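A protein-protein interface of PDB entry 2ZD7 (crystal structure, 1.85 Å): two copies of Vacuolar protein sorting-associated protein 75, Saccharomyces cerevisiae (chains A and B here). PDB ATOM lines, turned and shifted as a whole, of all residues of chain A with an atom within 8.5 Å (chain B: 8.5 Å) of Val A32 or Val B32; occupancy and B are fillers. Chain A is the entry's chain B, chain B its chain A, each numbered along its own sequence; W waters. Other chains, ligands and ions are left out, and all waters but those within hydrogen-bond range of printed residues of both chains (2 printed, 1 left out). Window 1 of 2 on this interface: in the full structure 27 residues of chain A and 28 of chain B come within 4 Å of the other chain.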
ATOM      1  N   VAL A  25     -18.018   2.308  -8.836  1.00  0.00           N
ATOM      2  CA  VAL A  25     -19.160   2.082  -7.958  1.00  0.00           C
ATOM      3  C   VAL A  25     -19.367   0.581  -7.735  1.00  0.00           C
ATOM      4  O   VAL A  25     -19.580   0.142  -6.606  1.00  0.00           O
ATOM      5  CB  VAL A  25     -20.449   2.714  -8.538  1.00  0.00           C
ATOM      6  CG1 VAL A  25     -21.664   2.270  -7.746  1.00  0.00           C
ATOM      7  CG2 VAL A  25     -20.341   4.239  -8.496  1.00  0.00           C
ATOM      8  N   ASP A  26     -19.294  -0.208  -8.802  1.00  0.00           N
ATOM      9  CA  ASP A  26     -19.466  -1.656  -8.658  1.00  0.00           C
ATOM     10  C   ASP A  26     -18.418  -2.201  -7.692  1.00  0.00           C
ATOM     11  O   ASP A  26     -18.721  -3.031  -6.837  1.00  0.00           O
ATOM     12  CB  ASP A  26     -19.318  -2.367 -10.008  1.00  0.00           C
ATOM     13  CG  ASP A  26     -20.418  -2.004 -10.987  1.00  0.00           C
ATOM     14  OD1 ASP A  26     -21.490  -1.551 -10.546  1.00  0.00           O
ATOM     15  OD2 ASP A  26     -20.208  -2.187 -12.204  1.00  0.00           O
ATOM     16  N   ALA A  27     -17.183  -1.725  -7.831  1.00  0.00           N
ATOM     17  CA  ALA A  27     -16.092  -2.172  -6.968  1.00  0.00           C
ATOM     18  C   ALA A  27     -16.365  -1.816  -5.514  1.00  0.00           C
ATOM     19  O   ALA A  27     -16.094  -2.608  -4.608  1.00  0.00           O
ATOM     20  CB  ALA A  27     -14.780  -1.556  -7.420  1.00  0.00           C
ATOM     21  N   ILE A  28     -16.891  -0.619  -5.282  1.00  0.00           N
ATOM     22  CA  ILE A  28     -17.205  -0.201  -3.925  1.00  0.00           C
ATOM     23  C   ILE A  28     -18.323  -1.078  -3.348  1.00  0.00           C
ATOM     24  O   ILE A  28     -18.259  -1.501  -2.186  1.00  0.00           O
ATOM     25  CB  ILE A  28     -17.630   1.291  -3.890  1.00  0.00           C
ATOM     26  CG1 ILE A  28     -16.400   2.178  -4.105  1.00  0.00           C
ATOM     27  CG2 ILE A  28     -18.308   1.620  -2.578  1.00  0.00           C
ATOM     28  CD1 ILE A  28     -16.739   3.669  -4.288  1.00  0.00           C
ATOM     29  N   GLU A  29     -19.346  -1.354  -4.150  1.00  0.00           N
ATOM     30  CA  GLU A  29     -20.456  -2.183  -3.678  1.00  0.00           C
ATOM     31  C   GLU A  29     -19.950  -3.547  -3.222  1.00  0.00           C
ATOM     32  O   GLU A  29     -20.425  -4.090  -2.224  1.00  0.00           O
ATOM     33  CB  GLU A  29     -21.512  -2.366  -4.770  1.00  0.00           C
ATOM     34  CG  GLU A  29     -22.365  -1.131  -5.043  1.00  0.00           C
ATOM     35  CD  GLU A  29     -23.086  -0.611  -3.804  1.00  0.00           C
ATOM     36  OE1 GLU A  29     -23.443  -1.422  -2.922  1.00  0.00           O
ATOM     37  OE2 GLU A  29     -23.317   0.612  -3.715  1.00  0.00           O
ATOM     38  N   ARG A  30     -18.990  -4.088  -3.965  1.00  0.00           N
ATOM     39  CA  ARG A  30     -18.388  -5.380  -3.645  1.00  0.00           C
ATOM     40  C   ARG A  30     -17.694  -5.292  -2.283  1.00  0.00           C
ATOM     41  O   ARG A  30     -17.947  -6.103  -1.394  1.00  0.00           O
ATOM     42  CB  ARG A  30     -17.374  -5.749  -4.731  1.00  0.00           C
ATOM     43  CG  ARG A  30     -16.317  -6.767  -4.321  1.00  0.00           C
ATOM     44  CD  ARG A  30     -16.771  -8.204  -4.522  1.00  0.00           C
ATOM     45  NE  ARG A  30     -15.736  -9.144  -4.085  1.00  0.00           N
ATOM     46  CZ  ARG A  30     -15.827 -10.465  -4.201  1.00  0.00           C
ATOM     47  NH1 ARG A  30     -16.906 -11.009  -4.745  1.00  0.00           N
ATOM     48  NH2 ARG A  30     -14.845 -11.240  -3.766  1.00  0.00           N
ATOM     49  N   GLU A  31     -16.822  -4.303  -2.124  1.00  0.00           N
ATOM     50  CA  GLU A  31     -16.104  -4.119  -0.865  1.00  0.00           C
ATOM     51  C   GLU A  31     -17.059  -3.896   0.301  1.00  0.00           C
ATOM     52  O   GLU A  31     -16.860  -4.447   1.386  1.00  0.00           O
ATOM     53  CB  GLU A  31     -15.145  -2.934  -0.966  1.00  0.00           C
ATOM     54  CG  GLU A  31     -13.968  -3.149  -1.899  1.00  0.00           C
ATOM     55  CD  GLU A  31     -13.036  -1.950  -1.928  1.00  0.00           C
ATOM     56  OE1 GLU A  31     -13.466  -0.877  -2.400  1.00  0.00           O
ATOM     57  OE2 GLU A  31     -11.879  -2.074  -1.472  1.00  0.00           O
ATOM     58  N   VAL A  32     -18.092  -3.085   0.079  1.00  0.00           N
ATOM     59  CA  VAL A  32     -19.079  -2.794   1.115  1.00  0.00           C
ATOM     60  C   VAL A  32     -19.829  -4.056   1.554  1.00  0.00           C
ATOM     61  O   VAL A  32     -20.059  -4.268   2.745  1.00  0.00           O
ATOM     62  CB  VAL A  32     -20.124  -1.759   0.631  1.00  0.00           C
ATOM     63  CG1 VAL A  32     -21.252  -1.647   1.637  1.00  0.00           C
ATOM     64  CG2 VAL A  32     -19.472  -0.409   0.440  1.00  0.00           C
ATOM     65  N   GLU A  33     -20.218  -4.888   0.593  1.00  0.00           N
ATOM     66  CA  GLU A  33     -20.939  -6.111   0.925  1.00  0.00           C
ATOM     67  C   GLU A  33     -20.048  -7.090   1.684  1.00  0.00           C
ATOM     68  O   GLU A  33     -20.494  -7.730   2.633  1.00  0.00           O
ATOM     69  CB  GLU A  33     -21.495  -6.762  -0.343  1.00  0.00           C
ATOM     70  CG  GLU A  33     -22.258  -8.067  -0.107  1.00  0.00           C
ATOM     71  CD  GLU A  33     -23.366  -7.951   0.931  1.00  0.00           C
ATOM     72  OE1 GLU A  33     -23.820  -6.823   1.225  1.00  0.00           O
ATOM     73  OE2 GLU A  33     -23.803  -9.004   1.447  1.00  0.00           O
ATOM     74  N   LEU A  34     -18.789  -7.199   1.270  1.00  0.00           N
ATOM     75  CA  LEU A  34     -17.844  -8.098   1.933  1.00  0.00           C
ATOM     76  C   LEU A  34     -17.606  -7.655   3.369  1.00  0.00           C
ATOM     77  O   LEU A  34     -17.424  -8.475   4.272  1.00  0.00           O
ATOM     78  CB  LEU A  34     -16.513  -8.119   1.177  1.00  0.00           C
ATOM     79  CG  LEU A  34     -16.313  -9.305   0.241  1.00  0.00           C
ATOM     80  CD1 LEU A  34     -15.047  -9.105  -0.563  1.00  0.00           C
ATOM     81  CD2 LEU A  34     -16.243 -10.593   1.070  1.00  0.00           C
ATOM     82  N   TYR A  35     -17.595  -6.340   3.563  1.00  0.00           N
ATOM     83  CA  TYR A  35     -17.406  -5.734   4.871  1.00  0.00           C
ATOM     84  C   TYR A  35     -18.605  -6.081   5.742  1.00  0.00           C
ATOM     85  O   TYR A  35     -18.458  -6.449   6.907  1.00  0.00           O
ATOM     86  CB  TYR A  35     -17.290  -4.218   4.696  1.00  0.00           C
ATOM     87  CG  TYR A  35     -17.117  -3.412   5.962  1.00  0.00           C
ATOM     88  CD1 TYR A  35     -16.041  -3.640   6.821  1.00  0.00           C
ATOM     89  CD2 TYR A  35     -17.991  -2.364   6.264  1.00  0.00           C
ATOM     90  CE1 TYR A  35     -15.837  -2.836   7.946  1.00  0.00           C
ATOM     91  CE2 TYR A  35     -17.794  -1.558   7.379  1.00  0.00           C
ATOM     92  CZ  TYR A  35     -16.715  -1.799   8.213  1.00  0.00           C
ATOM     93  OH  TYR A  35     -16.504  -0.984   9.304  1.00  0.00           O
ATOM     94  N   ARG A  36     -19.798  -5.980   5.168  1.00  0.00           N
ATOM     95  CA  ARG A  36     -21.011  -6.287   5.909  1.00  0.00           C
ATOM     96  C   ARG A  36     -21.053  -7.775   6.259  1.00  0.00           C
ATOM     97  O   ARG A  36     -21.375  -8.138   7.384  1.00  0.00           O
ATOM     98  CB  ARG A  36     -22.249  -5.916   5.086  1.00  0.00           C
ATOM     99  CG  ARG A  36     -23.570  -6.025   5.843  1.00  0.00           C
ATOM    100  CD  ARG A  36     -24.751  -5.745   4.923  1.00  0.00           C
ATOM    101  NE  ARG A  36     -24.954  -6.844   3.985  1.00  0.00           N
ATOM    102  CZ  ARG A  36     -25.509  -8.007   4.307  1.00  0.00           C
ATOM    103  NH1 ARG A  36     -25.928  -8.218   5.551  1.00  0.00           N
ATOM    104  NH2 ARG A  36     -25.627  -8.967   3.395  1.00  0.00           N
ATOM    105  N   LEU A  37     -20.715  -8.633   5.305  1.00  0.00           N
ATOM    106  CA  LEU A  37     -20.754 -10.077   5.567  1.00  0.00           C
ATOM    107  C   LEU A  37     -19.783 -10.498   6.676  1.00  0.00           C
ATOM    108  O   LEU A  37     -20.078 -11.405   7.465  1.00  0.00           O
ATOM    109  CB  LEU A  37     -20.449 -10.857   4.288  1.00  0.00           C
ATOM    110  CG  LEU A  37     -21.471 -10.692   3.160  1.00  0.00           C
ATOM    111  CD1 LEU A  37     -20.918 -11.324   1.899  1.00  0.00           C
ATOM    112  CD2 LEU A  37     -22.802 -11.314   3.553  1.00  0.00           C
ATOM    113  N   ASN A  38     -18.625  -9.848   6.719  1.00  0.00           N
ATOM    114  CA  ASN A  38     -17.618 -10.137   7.722  1.00  0.00           C
ATOM    115  C   ASN A  38     -18.110  -9.712   9.095  1.00  0.00           C
ATOM    116  O   ASN A  38     -17.960 -10.443  10.063  1.00  0.00           O
ATOM    117  CB  ASN A  38     -16.306  -9.413   7.398  1.00  0.00           C
ATOM    118  CG  ASN A  38     -15.369 -10.256   6.550  1.00  0.00           C
ATOM    119  OD1 ASN A  38     -14.921 -11.322   6.975  1.00  0.00           O
ATOM    120  ND2 ASN A  38     -15.064  -9.781   5.345  1.00  0.00           N
ATOM    121  N   LYS A  39     -18.700  -8.524   9.175  1.00  0.00           N
ATOM    122  CA  LYS A  39     -19.207  -8.017  10.440  1.00  0.00           C
ATOM    123  C   LYS A  39     -20.401  -8.819  10.967  1.00  0.00           C
ATOM    124  O   LYS A  39     -20.554  -8.995  12.179  1.00  0.00           O
ATOM    125  CB  LYS A  39     -19.612  -6.545  10.292  1.00  0.00           C
ATOM    126  CG  LYS A  39     -18.462  -5.558  10.446  1.00  0.00           C
ATOM    127  CD  LYS A  39     -18.964  -4.122  10.322  1.00  0.00           C
ATOM    128  CE  LYS A  39     -17.958  -3.117  10.872  1.00  0.00           C
ATOM    129  NZ  LYS A  39     -17.788  -3.247  12.341  1.00  0.00           N
ATOM    130  N   MET A  40     -21.242  -9.300  10.057  1.00  0.00           N
ATOM    131  CA  MET A  40     -22.427 -10.053  10.437  1.00  0.00           C
ATOM    132  C   MET A  40     -22.191 -11.495  10.882  1.00  0.00           C
ATOM    133  O   MET A  40     -22.970 -12.028  11.672  1.00  0.00           O
ATOM    134  CB  MET A  40     -23.447 -10.042   9.287  1.00  0.00           C
ATOM    135  CG  MET A  40     -24.112  -8.681   9.048  1.00  0.00           C
ATOM    136  SD  MET A  40     -25.210  -8.156  10.374  1.00  0.00           S
ATOM    137  CE  MET A  40     -26.567  -9.233  10.095  1.00  0.00           C
ATOM    138  N   THR A 100     -20.328 -12.257  -3.960  1.00  0.00           N
ATOM    139  CA  THR A 100     -20.835 -12.054  -2.607  1.00  0.00           C
ATOM    140  C   THR A 100     -22.222 -12.657  -2.448  1.00  0.00           C
ATOM    141  O   THR A 100     -22.772 -12.714  -1.348  1.00  0.00           O
ATOM    142  CB  THR A 100     -20.869 -10.555  -2.260  1.00  0.00           C
ATOM    143  OG1 THR A 100     -21.467  -9.823  -3.337  1.00  0.00           O
ATOM    144  CG2 THR A 100     -19.456 -10.048  -2.030  1.00  0.00           C
ATOM    145  N   VAL B  25     -27.102  -5.649  14.881  1.00  0.00           N
ATOM    146  CA  VAL B  25     -27.267  -5.614  13.433  1.00  0.00           C
ATOM    147  C   VAL B  25     -27.495  -4.165  13.004  1.00  0.00           C
ATOM    148  O   VAL B  25     -26.939  -3.716  12.002  1.00  0.00           O
ATOM    149  CB  VAL B  25     -28.469  -6.469  12.984  1.00  0.00           C
ATOM    150  CG1 VAL B  25     -28.726  -6.269  11.489  1.00  0.00           C
ATOM    151  CG2 VAL B  25     -28.200  -7.941  13.289  1.00  0.00           C
ATOM    152  N   ASP B  26     -28.308  -3.435  13.767  1.00  0.00           N
ATOM    153  CA  ASP B  26     -28.582  -2.034  13.446  1.00  0.00           C
ATOM    154  C   ASP B  26     -27.288  -1.229  13.473  1.00  0.00           C
ATOM    155  O   ASP B  26     -27.067  -0.369  12.617  1.00  0.00           O
ATOM    156  CB  ASP B  26     -29.576  -1.410  14.432  1.00  0.00           C
ATOM    157  CG  ASP B  26     -30.977  -1.989  14.310  1.00  0.00           C
ATOM    158  OD1 ASP B  26     -31.320  -2.556  13.252  1.00  0.00           O
ATOM    159  OD2 ASP B  26     -31.749  -1.859  15.283  1.00  0.00           O
ATOM    160  N   ALA B  27     -26.437  -1.504  14.459  1.00  0.00           N
ATOM    161  CA  ALA B  27     -25.167  -0.801  14.572  1.00  0.00           C
ATOM    162  C   ALA B  27     -24.280  -1.134  13.373  1.00  0.00           C
ATOM    163  O   ALA B  27     -23.617  -0.259  12.809  1.00  0.00           O
ATOM    164  CB  ALA B  27     -24.459  -1.176  15.881  1.00  0.00           C
ATOM    165  N   ILE B  28     -24.272  -2.403  12.977  1.00  0.00           N
ATOM    166  CA  ILE B  28     -23.471  -2.822  11.837  1.00  0.00           C
ATOM    167  C   ILE B  28     -23.945  -2.137  10.553  1.00  0.00           C
ATOM    168  O   ILE B  28     -23.129  -1.667   9.763  1.00  0.00           O
ATOM    169  CB  ILE B  28     -23.528  -4.359  11.656  1.00  0.00           C
ATOM    170  CG1 ILE B  28     -22.736  -5.032  12.780  1.00  0.00           C
ATOM    171  CG2 ILE B  28     -22.951  -4.762  10.305  1.00  0.00           C
ATOM    172  CD1 ILE B  28     -22.922  -6.540  12.836  1.00  0.00           C
ATOM    173  N   GLU B  29     -25.260  -2.087  10.347  1.00  0.00           N
ATOM    174  CA  GLU B  29     -25.813  -1.454   9.153  1.00  0.00           C
ATOM    175  C   GLU B  29     -25.339  -0.009   9.050  1.00  0.00           C
ATOM    176  O   GLU B  29     -24.974   0.457   7.970  1.00  0.00           O
ATOM    177  CB  GLU B  29     -27.342  -1.486   9.181  1.00  0.00           C
ATOM    178  CG  GLU B  29     -27.950  -2.874   9.062  1.00  0.00           C
ATOM    179  CD  GLU B  29     -27.773  -3.475   7.683  1.00  0.00           C
ATOM    180  OE1 GLU B  29     -26.620  -3.594   7.218  1.00  0.00           O
ATOM    181  OE2 GLU B  29     -28.794  -3.833   7.060  1.00  0.00           O
ATOM    182  N   ARG B  30     -25.336   0.706  10.170  1.00  0.00           N
ATOM    183  CA  ARG B  30     -24.890   2.096  10.147  1.00  0.00           C
ATOM    184  C   ARG B  30     -23.405   2.170   9.797  1.00  0.00           C
ATOM    185  O   ARG B  30     -23.003   2.954   8.945  1.00  0.00           O
ATOM    186  CB  ARG B  30     -25.135   2.786  11.495  1.00  0.00           C
ATOM    187  CG  ARG B  30     -24.662   4.245  11.492  1.00  0.00           C
ATOM    188  CD  ARG B  30     -24.819   4.948  12.833  1.00  0.00           C
ATOM    189  NE  ARG B  30     -24.145   6.247  12.826  1.00  0.00           N
ATOM    190  CZ  ARG B  30     -24.679   7.378  12.364  1.00  0.00           C
ATOM    191  NH1 ARG B  30     -25.908   7.393  11.869  1.00  0.00           N
ATOM    192  NH2 ARG B  30     -23.973   8.502  12.391  1.00  0.00           N
ATOM    193  N   GLU B  31     -22.588   1.343  10.443  1.00  0.00           N
ATOM    194  CA  GLU B  31     -21.150   1.350  10.166  1.00  0.00           C
ATOM    195  C   GLU B  31     -20.873   1.068   8.680  1.00  0.00           C
ATOM    196  O   GLU B  31     -20.015   1.699   8.053  1.00  0.00           O
ATOM    197  CB  GLU B  31     -20.449   0.308  11.055  1.00  0.00           C
ATOM    198  CG  GLU B  31     -20.857   0.443  12.527  1.00  0.00           C
ATOM    199  CD  GLU B  31     -20.200  -0.563  13.461  1.00  0.00           C
ATOM    200  OE1 GLU B  31     -20.109  -1.757  13.105  1.00  0.00           O
ATOM    201  OE2 GLU B  31     -19.789  -0.156  14.570  1.00  0.00           O
ATOM    202  N   VAL B  32     -21.615   0.124   8.118  1.00  0.00           N
ATOM    203  CA  VAL B  32     -21.447  -0.244   6.722  1.00  0.00           C
ATOM    204  C   VAL B  32     -21.871   0.908   5.807  1.00  0.00           C
ATOM    205  O   VAL B  32     -21.208   1.202   4.816  1.00  0.00           O
ATOM    206  CB  VAL B  32     -22.282  -1.502   6.388  1.00  0.00           C
ATOM    207  CG1 VAL B  32     -22.255  -1.779   4.887  1.00  0.00           C
ATOM    208  CG2 VAL B  32     -21.722  -2.714   7.153  1.00  0.00           C
ATOM    209  N   GLU B  33     -22.966   1.571   6.151  1.00  0.00           N
ATOM    210  CA  GLU B  33     -23.432   2.667   5.317  1.00  0.00           C
ATOM    211  C   GLU B  33     -22.477   3.860   5.359  1.00  0.00           C
ATOM    212  O   GLU B  33     -22.287   4.513   4.340  1.00  0.00           O
ATOM    213  CB  GLU B  33     -24.848   3.091   5.718  1.00  0.00           C
ATOM    214  CG  GLU B  33     -25.403   4.258   4.890  1.00  0.00           C
ATOM    215  CD  GLU B  33     -25.657   3.930   3.414  1.00  0.00           C
ATOM    216  OE1 GLU B  33     -25.375   2.798   2.963  1.00  0.00           O
ATOM    217  OE2 GLU B  33     -26.147   4.831   2.697  1.00  0.00           O
ATOM    218  N   LEU B  34     -21.878   4.141   6.520  1.00  0.00           N
ATOM    219  CA  LEU B  34     -20.930   5.257   6.629  1.00  0.00           C
ATOM    220  C   LEU B  34     -19.703   4.970   5.771  1.00  0.00           C
ATOM    221  O   LEU B  34     -19.147   5.873   5.142  1.00  0.00           O
ATOM    222  CB  LEU B  34     -20.496   5.487   8.090  1.00  0.00           C
ATOM    223  CG  LEU B  34     -21.493   6.179   9.023  1.00  0.00           C
ATOM    224  CD1 LEU B  34     -20.993   6.146  10.472  1.00  0.00           C
ATOM    225  CD2 LEU B  34     -21.680   7.617   8.556  1.00  0.00           C
ATOM    226  N   TYR B  35     -19.266   3.714   5.762  1.00  0.00           N
ATOM    227  CA  TYR B  35     -18.124   3.300   4.951  1.00  0.00           C
ATOM    228  C   TYR B  35     -18.459   3.516   3.465  1.00  0.00           C
ATOM    229  O   TYR B  35     -17.672   4.090   2.700  1.00  0.00           O
ATOM    230  CB  TYR B  35     -17.815   1.815   5.220  1.00  0.00           C
ATOM    231  CG  TYR B  35     -16.844   1.167   4.250  1.00  0.00           C
ATOM    232  CD1 TYR B  35     -15.611   1.750   3.959  1.00  0.00           C
ATOM    233  CD2 TYR B  35     -17.153  -0.052   3.643  1.00  0.00           C
ATOM    234  CE1 TYR B  35     -14.703   1.134   3.088  1.00  0.00           C
ATOM    235  CE2 TYR B  35     -16.259  -0.679   2.776  1.00  0.00           C
ATOM    236  CZ  TYR B  35     -15.036  -0.083   2.503  1.00  0.00           C
ATOM    237  OH  TYR B  35     -14.148  -0.725   1.668  1.00  0.00           O
ATOM    238  N   ARG B  36     -19.637   3.062   3.057  1.00  0.00           N
ATOM    239  CA  ARG B  36     -20.039   3.217   1.670  1.00  0.00           C
ATOM    240  C   ARG B  36     -20.129   4.684   1.296  1.00  0.00           C
ATOM    241  O   ARG B  36     -19.654   5.082   0.245  1.00  0.00           O
ATOM    242  CB  ARG B  36     -21.405   2.574   1.420  1.00  0.00           C
ATOM    243  CG  ARG B  36     -21.801   2.570  -0.054  1.00  0.00           C
ATOM    244  CD  ARG B  36     -23.212   1.987  -0.245  1.00  0.00           C
ATOM    245  NE  ARG B  36     -24.250   2.914   0.194  1.00  0.00           N
ATOM    246  CZ  ARG B  36     -24.664   3.971  -0.506  1.00  0.00           C
ATOM    247  NH1 ARG B  36     -24.125   4.240  -1.690  1.00  0.00           N
ATOM    248  NH2 ARG B  36     -25.624   4.760  -0.025  1.00  0.00           N
ATOM    249  N   LEU B  37     -20.735   5.490   2.157  1.00  0.00           N
ATOM    250  CA  LEU B  37     -20.892   6.909   1.834  1.00  0.00           C
ATOM    251  C   LEU B  37     -19.549   7.635   1.737  1.00  0.00           C
ATOM    252  O   LEU B  37     -19.370   8.512   0.884  1.00  0.00           O
ATOM    253  CB  LEU B  37     -21.804   7.600   2.858  1.00  0.00           C
ATOM    254  CG  LEU B  37     -23.284   7.193   2.812  1.00  0.00           C
ATOM    255  CD1 LEU B  37     -23.993   7.771   4.009  1.00  0.00           C
ATOM    256  CD2 LEU B  37     -23.938   7.697   1.512  1.00  0.00           C
ATOM    257  N   ASN B  38     -18.600   7.280   2.600  1.00  0.00           N
ATOM    258  CA  ASN B  38     -17.283   7.923   2.556  1.00  0.00           C
ATOM    259  C   ASN B  38     -16.506   7.544   1.292  1.00  0.00           C
ATOM    260  O   ASN B  38     -15.864   8.394   0.667  1.00  0.00           O
ATOM    261  CB  ASN B  38     -16.474   7.564   3.821  1.00  0.00           C
ATOM    262  CG  ASN B  38     -16.823   8.452   5.014  1.00  0.00           C
ATOM    263  OD1 ASN B  38     -16.453   9.629   5.053  1.00  0.00           O
ATOM    264  ND2 ASN B  38     -17.535   7.895   5.995  1.00  0.00           N
ATOM    265  N   LYS B  39     -16.552   6.269   0.918  1.00  0.00           N
ATOM    266  CA  LYS B  39     -15.868   5.799  -0.279  1.00  0.00           C
ATOM    267  C   LYS B  39     -16.508   6.368  -1.547  1.00  0.00           C
ATOM    268  O   LYS B  39     -15.822   6.639  -2.537  1.00  0.00           O
ATOM    269  CB  LYS B  39     -15.922   4.269  -0.373  1.00  0.00           C
ATOM    270  CG  LYS B  39     -14.575   3.583  -0.208  1.00  0.00           C
ATOM    271  CD  LYS B  39     -14.530   2.287  -1.002  1.00  0.00           C
ATOM    272  CE  LYS B  39     -13.189   1.601  -0.882  1.00  0.00           C
ATOM    273  NZ  LYS B  39     -12.045   2.501  -1.172  1.00  0.00           N
ATOM    274  N   MET B  40     -17.827   6.525  -1.506  1.00  0.00           N
ATOM    275  CA  MET B  40     -18.589   7.015  -2.654  1.00  0.00           C
ATOM    276  C   MET B  40     -18.453   8.529  -2.882  1.00  0.00           C
ATOM    277  O   MET B  40     -18.498   9.000  -4.015  1.00  0.00           O
ATOM    278  CB  MET B  40     -20.067   6.633  -2.459  1.00  0.00           C
ATOM    279  CG  MET B  40     -20.822   6.204  -3.714  1.00  0.00           C
ATOM    280  SD  MET B  40     -20.245   4.721  -4.558  1.00  0.00           S
ATOM    281  CE  MET B  40     -19.279   5.414  -5.684  1.00  0.00           C
ATOM    282  N   THR B 100     -28.153   8.202   8.932  1.00  0.00           N
ATOM    283  CA  THR B 100     -27.550   7.874   7.652  1.00  0.00           C
ATOM    284  C   THR B 100     -28.421   8.297   6.455  1.00  0.00           C
ATOM    285  O   THR B 100     -27.931   8.434   5.325  1.00  0.00           O
ATOM    286  CB  THR B 100     -27.254   6.354   7.619  1.00  0.00           C
ATOM    287  OG1 THR B 100     -25.850   6.144   7.834  1.00  0.00           O
ATOM    288  CG2 THR B 100     -27.693   5.737   6.324  1.00  0.00           C
HETATM  289  O   HOH W   1     -26.829  -6.475   8.022  1.00  0.00           O
HETATM  290  O   HOH W   2     -11.769   0.094   0.951  1.00  0.00           O
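The side-chain carboxylate of Glu B31 lies within salt-bridge range of the side-chain amino group of Lys A39 (2.9 Å). The side-chain carboxylate (OE1) of Glu A31 is in salt-bridge range of the side-chain amino group (NZ) of Lys B39, at 3.9 Å.
The guanidinium group (NH2) of Arg B36 lies within salt-bridge range of the side-chain carboxylate (OE2) of Glu B33. The side-chain carboxylate (OE2) of Glu A33 is in salt-bridge range of the guanidinium group (NH2) of Arg A36, 2.7 Å away.
Among the printed residues, merely in contact across the chains: Val A25 with Met B40, Ile A28 with Met B40, Val A32 with Val B32, Lys A39 with Ile B28, Ile A28 with Lys B39, Glu A31 with Tyr B35, Tyr A35 with Tyr B35, Arg A36 with Glu B29, Val A32 with Arg B36, Met A40 with Ile B28, Glu A29 with Arg B36, Met A40 with Val B25, Arg A36 with Val B32, Tyr A35 with Val B32, Val A32 with Tyr B35 and Tyr A35 with Glu B31.
Asp A26 touches none of the printed residues of chain B. Of the printed residues of chain B, Ile A28 touches Lys B39 and Met B40. Val A32 touches just these residues of chain B: Val B32 (3.4 Å), Tyr B35 (3.9 Å) and Arg B36 (3.7 Å). Of the printed residues of chain B, Tyr A35 touches Glu B31, Val B32 and Tyr B35. Of the printed residues of chain A, Glu B29 touches Arg A36. Arg B30 touches none of the printed residues of chain A. Val B32 touches just these residues of chain A: Val A32 (3.4 Å), Tyr A35 (3.9 Å) and Arg A36 (3.8 Å). The nearest printed residue of chain B that does not touch Val A32 is Glu B33 (5.8 Å). The nearest printed residue of chain A that does not touch Ile B28 is Arg A36 (4.7 Å).
Printed residues of chain A that touch a printed residue of chain B: Val A25, Ile A28, Glu A29, Glu A31, Val A32, Tyr A35, Arg A36, Lys A39 and Met A40. Hydrophobic or aromatic side chains of chain A that line the printed part of chain B: Val A25, Ile A28, Val A32, Tyr A35 and Met A40. Printed residues of chain B that touch a printed residue of chain A: Val B25, Ile B28, Glu B29, Glu B31, Val B32, Tyr B35, Arg B36, Lys B39 and Met B40. Hydrophobic or aromatic side chains of chain B that line the printed part of chain A: Val B25, Ile B28, Val B32, Tyr B35 and Met B40.
Val A25 touches Met B40, and with the chains exchanged Met A40 touches Val B25. Ile A28 touches Met B40, and with the chains exchanged Met A40 touches Ile B28. Val B32 touches its own counterpart, Val A32. Val A32 touches Arg B36, and with the chains exchanged Arg A36 touches Val B32.
Water W2 lies within hydrogen-bond range of the side-chain hydroxyl of Tyr B35 (2.6 Å), the side-chain amino group of Lys B39 (3.2 Å) and the side-chain carboxylate of Glu A31 (3.3 Å). Water W1 lies within hydrogen-bond range of OE1 of Glu B29, NH1 of Arg A36 and SD of Met A40.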
